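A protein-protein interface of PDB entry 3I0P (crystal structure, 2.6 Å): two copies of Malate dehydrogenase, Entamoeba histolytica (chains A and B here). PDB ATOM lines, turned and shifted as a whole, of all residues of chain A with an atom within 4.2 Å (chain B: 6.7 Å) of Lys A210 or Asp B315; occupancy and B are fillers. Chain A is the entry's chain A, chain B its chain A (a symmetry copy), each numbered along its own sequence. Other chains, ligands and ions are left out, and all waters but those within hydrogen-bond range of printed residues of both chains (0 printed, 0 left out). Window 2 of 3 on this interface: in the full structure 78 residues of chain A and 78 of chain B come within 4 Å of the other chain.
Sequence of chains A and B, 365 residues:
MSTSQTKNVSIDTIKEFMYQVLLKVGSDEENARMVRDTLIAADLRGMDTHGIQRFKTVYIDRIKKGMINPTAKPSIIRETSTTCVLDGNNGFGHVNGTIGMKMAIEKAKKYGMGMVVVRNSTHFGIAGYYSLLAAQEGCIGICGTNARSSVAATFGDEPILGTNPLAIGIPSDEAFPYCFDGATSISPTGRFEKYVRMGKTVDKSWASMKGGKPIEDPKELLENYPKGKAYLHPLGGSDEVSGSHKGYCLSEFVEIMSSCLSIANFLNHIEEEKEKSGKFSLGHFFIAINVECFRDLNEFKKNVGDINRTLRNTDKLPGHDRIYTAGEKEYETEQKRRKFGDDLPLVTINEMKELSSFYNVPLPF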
ATOM      1  N   PHE A 155     -16.578  -8.253 -17.892  1.00  0.00           N
ATOM      2  CA  PHE A 155     -16.399  -9.608 -18.458  1.00  0.00           C
ATOM      3  C   PHE A 155     -15.048  -9.780 -19.167  1.00  0.00           C
ATOM      4  O   PHE A 155     -14.839 -10.770 -19.878  1.00  0.00           O
ATOM      5  CB  PHE A 155     -17.561 -10.036 -19.386  1.00  0.00           C
ATOM      6  CG  PHE A 155     -18.930  -9.910 -18.763  1.00  0.00           C
ATOM      7  CD1 PHE A 155     -19.141 -10.209 -17.414  1.00  0.00           C
ATOM      8  CD2 PHE A 155     -20.021  -9.511 -19.540  1.00  0.00           C
ATOM      9  CE1 PHE A 155     -20.412 -10.087 -16.843  1.00  0.00           C
ATOM     10  CE2 PHE A 155     -21.300  -9.389 -18.983  1.00  0.00           C
ATOM     11  CZ  PHE A 155     -21.495  -9.675 -17.632  1.00  0.00           C
ATOM     12  N   GLY A 156     -14.140  -8.822 -18.965  1.00  0.00           N
ATOM     13  CA  GLY A 156     -12.835  -8.814 -19.638  1.00  0.00           C
ATOM     14  C   GLY A 156     -11.740  -9.384 -18.763  1.00  0.00           C
ATOM     15  O   GLY A 156     -11.853  -9.376 -17.534  1.00  0.00           O
ATOM     16  N   ASP A 157     -10.679  -9.884 -19.397  1.00  0.00           N
ATOM     17  CA  ASP A 157      -9.588 -10.579 -18.696  1.00  0.00           C
ATOM     18  C   ASP A 157      -8.237  -9.988 -19.114  1.00  0.00           C
ATOM     19  O   ASP A 157      -7.200 -10.667 -19.094  1.00  0.00           O
ATOM     20  CB  ASP A 157      -9.653 -12.087 -19.000  1.00  0.00           C
ATOM     21  CG  ASP A 157      -8.982 -12.950 -17.925  1.00  0.00           C
ATOM     22  OD1 ASP A 157      -8.974 -12.549 -16.741  1.00  0.00           O
ATOM     23  OD2 ASP A 157      -8.468 -14.040 -18.267  1.00  0.00           O
ATOM     24  N   GLU A 158      -8.259  -8.704 -19.460  1.00  0.00           N
ATOM     25  CA  GLU A 158      -7.154  -8.045 -20.147  1.00  0.00           C
ATOM     26  C   GLU A 158      -7.276  -6.523 -19.961  1.00  0.00           C
ATOM     27  O   GLU A 158      -8.366  -5.975 -20.106  1.00  0.00           O
ATOM     28  CB  GLU A 158      -7.230  -8.402 -21.635  1.00  0.00           C
ATOM     29  CG  GLU A 158      -5.979  -8.104 -22.454  1.00  0.00           C
ATOM     30  CD  GLU A 158      -6.227  -8.155 -23.969  1.00  0.00           C
ATOM     31  OE1 GLU A 158      -7.275  -8.684 -24.416  1.00  0.00           O
ATOM     32  OE2 GLU A 158      -5.354  -7.657 -24.716  1.00  0.00           O
ATOM     33  N   SER A 208      -7.003  -7.616 -10.355  1.00  0.00           N
ATOM     34  CA  SER A 208      -6.994  -9.062 -10.505  1.00  0.00           C
ATOM     35  C   SER A 208      -5.876  -9.511 -11.437  1.00  0.00           C
ATOM     36  O   SER A 208      -5.467  -8.767 -12.337  1.00  0.00           O
ATOM     37  CB  SER A 208      -8.347  -9.561 -11.021  1.00  0.00           C
ATOM     38  OG  SER A 208      -9.338  -9.495 -10.010  1.00  0.00           O
ATOM     39  N   MET A 209      -5.363 -10.717 -11.200  1.00  0.00           N
ATOM     40  CA  MET A 209      -4.420 -11.344 -12.119  1.00  0.00           C
ATOM     41  C   MET A 209      -5.237 -11.889 -13.277  1.00  0.00           C
ATOM     42  O   MET A 209      -6.441 -12.076 -13.141  1.00  0.00           O
ATOM     43  CB  MET A 209      -3.644 -12.478 -11.429  1.00  0.00           C
ATOM     44  CG  MET A 209      -2.533 -12.036 -10.445  1.00  0.00           C
ATOM     45  SD  MET A 209      -1.077 -11.215 -11.167  1.00  0.00           S
ATOM     46  CE  MET A 209      -0.557 -12.379 -12.432  1.00  0.00           C
ATOM     47  N   LYS A 210      -4.592 -12.122 -14.418  1.00  0.00           N
ATOM     48  CA  LYS A 210      -5.236 -12.806 -15.537  1.00  0.00           C
ATOM     49  C   LYS A 210      -5.963 -14.034 -14.990  1.00  0.00           C
ATOM     50  O   LYS A 210      -5.404 -14.784 -14.181  1.00  0.00           O
ATOM     51  CB  LYS A 210      -4.192 -13.214 -16.579  1.00  0.00           C
ATOM     52  CG  LYS A 210      -4.733 -13.936 -17.804  1.00  0.00           C
ATOM     53  CD  LYS A 210      -4.951 -12.994 -18.950  1.00  0.00           C
ATOM     54  CE  LYS A 210      -5.177 -13.757 -20.235  1.00  0.00           C
ATOM     55  NZ  LYS A 210      -5.283 -12.817 -21.384  1.00  0.00           N
ATOM     56  N   GLY A 211      -7.217 -14.214 -15.403  1.00  0.00           N
ATOM     57  CA  GLY A 211      -8.059 -15.295 -14.881  1.00  0.00           C
ATOM     58  C   GLY A 211      -9.000 -14.884 -13.763  1.00  0.00           C
ATOM     59  O   GLY A 211      -9.864 -15.660 -13.359  1.00  0.00           O
ATOM     60  N   GLY A 212      -8.825 -13.671 -13.249  1.00  0.00           N
ATOM     61  CA  GLY A 212      -9.765 -13.094 -12.285  1.00  0.00           C
ATOM     62  C   GLY A 212      -9.447 -13.257 -10.808  1.00  0.00           C
ATOM     63  O   GLY A 212     -10.258 -12.882  -9.958  1.00  0.00           O
ATOM     64  N   LYS A 229      -1.159  -9.047 -18.493  1.00  0.00           N
ATOM     65  CA  LYS A 229      -1.442 -10.229 -17.669  1.00  0.00           C
ATOM     66  C   LYS A 229      -2.063  -9.901 -16.294  1.00  0.00           C
ATOM     67  O   LYS A 229      -2.276 -10.796 -15.474  1.00  0.00           O
ATOM     68  CB  LYS A 229      -0.191 -11.126 -17.529  1.00  0.00           C
ATOM     69  N   LEU B 311     -12.985  -3.216 -27.705  1.00  0.00           N
ATOM     70  CA  LEU B 311     -13.421  -3.625 -26.371  1.00  0.00           C
ATOM     71  C   LEU B 311     -13.983  -5.050 -26.377  1.00  0.00           C
ATOM     72  O   LEU B 311     -13.555  -5.891 -25.577  1.00  0.00           O
ATOM     73  CB  LEU B 311     -14.437  -2.627 -25.793  1.00  0.00           C
ATOM     74  CG  LEU B 311     -13.923  -1.267 -25.282  1.00  0.00           C
ATOM     75  CD1 LEU B 311     -15.098  -0.361 -24.936  1.00  0.00           C
ATOM     76  CD2 LEU B 311     -12.981  -1.412 -24.080  1.00  0.00           C
ATOM     77  N   ARG B 312     -14.906  -5.316 -27.304  1.00  0.00           N
ATOM     78  CA  ARG B 312     -15.542  -6.637 -27.429  1.00  0.00           C
ATOM     79  C   ARG B 312     -14.576  -7.757 -27.837  1.00  0.00           C
ATOM     80  O   ARG B 312     -14.815  -8.929 -27.520  1.00  0.00           O
ATOM     81  CB  ARG B 312     -16.726  -6.574 -28.396  1.00  0.00           C
ATOM     82  CG  ARG B 312     -17.913  -5.835 -27.828  1.00  0.00           C
ATOM     83  CD  ARG B 312     -19.103  -5.953 -28.725  1.00  0.00           C
ATOM     84  NE  ARG B 312     -19.141  -4.894 -29.725  1.00  0.00           N
ATOM     85  CZ  ARG B 312     -19.966  -3.854 -29.683  1.00  0.00           C
ATOM     86  NH1 ARG B 312     -19.942  -2.952 -30.643  1.00  0.00           N
ATOM     87  NH2 ARG B 312     -20.824  -3.712 -28.691  1.00  0.00           N
ATOM     88  N   ASN B 313     -13.491  -7.388 -28.521  1.00  0.00           N
ATOM     89  CA  ASN B 313     -12.461  -8.335 -28.944  1.00  0.00           C
ATOM     90  C   ASN B 313     -11.410  -8.730 -27.909  1.00  0.00           C
ATOM     91  O   ASN B 313     -10.584  -9.594 -28.194  1.00  0.00           O
ATOM     92  CB  ASN B 313     -11.740  -7.816 -30.183  1.00  0.00           C
ATOM     93  CG  ASN B 313     -12.225  -8.470 -31.455  1.00  0.00           C
ATOM     94  OD1 ASN B 313     -12.382  -9.696 -31.527  1.00  0.00           O
ATOM     95  ND2 ASN B 313     -12.450  -7.658 -32.479  1.00  0.00           N
ATOM     96  N   THR B 314     -11.417  -8.103 -26.731  1.00  0.00           N
ATOM     97  CA  THR B 314     -10.435  -8.436 -25.690  1.00  0.00           C
ATOM     98  C   THR B 314     -10.774  -9.766 -25.019  1.00  0.00           C
ATOM     99  O   THR B 314     -11.904 -10.244 -25.114  1.00  0.00           O
ATOM    100  CB  THR B 314     -10.274  -7.318 -24.617  1.00  0.00           C
ATOM    101  OG1 THR B 314     -11.546  -7.001 -24.038  1.00  0.00           O
ATOM    102  CG2 THR B 314      -9.664  -6.068 -25.223  1.00  0.00           C
ATOM    103  N   ASP B 315      -9.792 -10.365 -24.351  1.00  0.00           N
ATOM    104  CA  ASP B 315      -9.977 -11.680 -23.746  1.00  0.00           C
ATOM    105  C   ASP B 315     -11.120 -11.675 -22.739  1.00  0.00           C
ATOM    106  O   ASP B 315     -11.177 -10.827 -21.847  1.00  0.00           O
ATOM    107  CB  ASP B 315      -8.686 -12.182 -23.089  1.00  0.00           C
ATOM    108  CG  ASP B 315      -7.597 -12.522 -24.102  1.00  0.00           C
ATOM    109  OD1 ASP B 315      -7.922 -12.824 -25.280  1.00  0.00           O
ATOM    110  OD2 ASP B 315      -6.409 -12.493 -23.710  1.00  0.00           O
ATOM    111  N   LYS B 316     -12.029 -12.629 -22.909  1.00  0.00           N
ATOM    112  CA  LYS B 316     -13.190 -12.772 -22.042  1.00  0.00           C
ATOM    113  C   LYS B 316     -12.871 -13.628 -20.813  1.00  0.00           C
ATOM    114  O   LYS B 316     -12.237 -14.684 -20.915  1.00  0.00           O
ATOM    115  CB  LYS B 316     -14.363 -13.344 -22.843  1.00  0.00           C
ATOM    116  CG  LYS B 316     -15.101 -12.287 -23.661  1.00  0.00           C
ATOM    117  CD  LYS B 316     -15.388 -12.732 -25.072  1.00  0.00           C
ATOM    118  CE  LYS B 316     -14.343 -12.223 -26.047  1.00  0.00           C
ATOM    119  NZ  LYS B 316     -14.759 -12.418 -27.475  1.00  0.00           N
ATOM    120  N   LEU B 317     -13.294 -13.147 -19.649  1.00  0.00           N
ATOM    121  CA  LEU B 317     -13.152 -13.878 -18.392  1.00  0.00           C
ATOM    122  C   LEU B 317     -13.863 -15.226 -18.516  1.00  0.00           C
ATOM    123  O   LEU B 317     -14.997 -15.278 -19.009  1.00  0.00           O
ATOM    124  CB  LEU B 317     -13.759 -13.051 -17.250  1.00  0.00           C
ATOM    125  CG  LEU B 317     -13.559 -13.395 -15.770  1.00  0.00           C
ATOM    126  CD1 LEU B 317     -12.088 -13.402 -15.384  1.00  0.00           C
ATOM    127  CD2 LEU B 317     -14.349 -12.412 -14.894  1.00  0.00           C
ATOM    128  N   ILE B 323     -18.526  -9.664 -24.260  1.00  0.00           N
ATOM    129  CA  ILE B 323     -18.421  -8.352 -23.654  1.00  0.00           C
ATOM    130  C   ILE B 323     -19.418  -7.446 -24.385  1.00  0.00           C
ATOM    131  O   ILE B 323     -19.545  -7.514 -25.605  1.00  0.00           O
ATOM    132  CB  ILE B 323     -16.961  -7.818 -23.756  1.00  0.00           C
ATOM    133  CG1 ILE B 323     -16.029  -8.683 -22.894  1.00  0.00           C
ATOM    134  CG2 ILE B 323     -16.866  -6.332 -23.369  1.00  0.00           C
ATOM    135  CD1 ILE B 323     -14.536  -8.507 -23.163  1.00  0.00           C
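NZ of Lys A210 is in salt-bridge range of OD2 of Asp B315 (2.6 Å). The backbone NH of Asp A157 sits at hydrogen-bond distance from the backbone carbonyl oxygen of Asp B315 (2.7 Å). The backbone carbonyl oxygen (O) of Phe A155 is in hydrogen-bond range of the backbone NH (N) of Leu B317, at 2.8 Å. OE1 of Glu A158 lies within hydrogen-bond range of N of Asp B315, at 3.0 Å.
The backbone carbonyl oxygen of Lys A229 sits at hydrogen-bond distance from the backbone NH of Lys A210. The side-chain carboxylate (OD1) of Asp A157 is in hydrogen-bond range of the backbone NH (N) of Gly A211 (2.8 Å). The backbone carbonyl oxygen (O) of Leu B311 is in hydrogen-bond range of the side-chain hydroxyl (OG1) of Thr B314 (2.8 Å). O of Arg B312 sits at hydrogen-bond distance from NZ of Lys B316 (3.5 Å).
Among the printed residues, merely in contact across the chains: Glu A158 with Thr B314, Phe A155 with Lys B316, Gly A156 with Asp B315, Asp A157 with Leu B317, Gly A211 with Leu B317, Phe A155 with Ile B323, Gly A212 with Leu B317 and Gly A156 with Ile B323.
Of chain B, only Asp B315 (2.6 Å) comes within 4 Å of Lys A210. Asp B315 touches just these residues of chain A: Gly A156 (3.4 Å), Asp A157 (2.7 Å), Glu A158 (3.0 Å) and Lys A210 (2.6 Å). Of the printed residues of chain B, Asp A157 touches Asp B315 and Leu B317. Printed residues of chain B within 4 Å of Phe A155: Lys B316, Leu B317 and Ile B323. The nearest residue of chain B that does not touch Lys A210 is Leu B317 (6.2 Å). The nearest printed residue of chain A that does not touch Asp B315 is Phe A155 (4.2 Å). The nearest printed residue of chain B that does not touch Phe A155 is Asp B315 (4.2 Å).
Printed residues of chain B that touch a printed residue of chain A: Thr B314, Asp B315, Lys B316, Leu B317 and Ile B323. Hydrophobic or aromatic side chains of chain B within 4 Å of the printed part of chain A: Leu B317 and Ile B323. Along chain B the printed residues that touch a printed residue of chain A span positions 314 to 323.
No position is printed for both chains. Of the 12 pairs that touch across the chains among the printed residues, none has its exchanged pair printed and touching as well.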
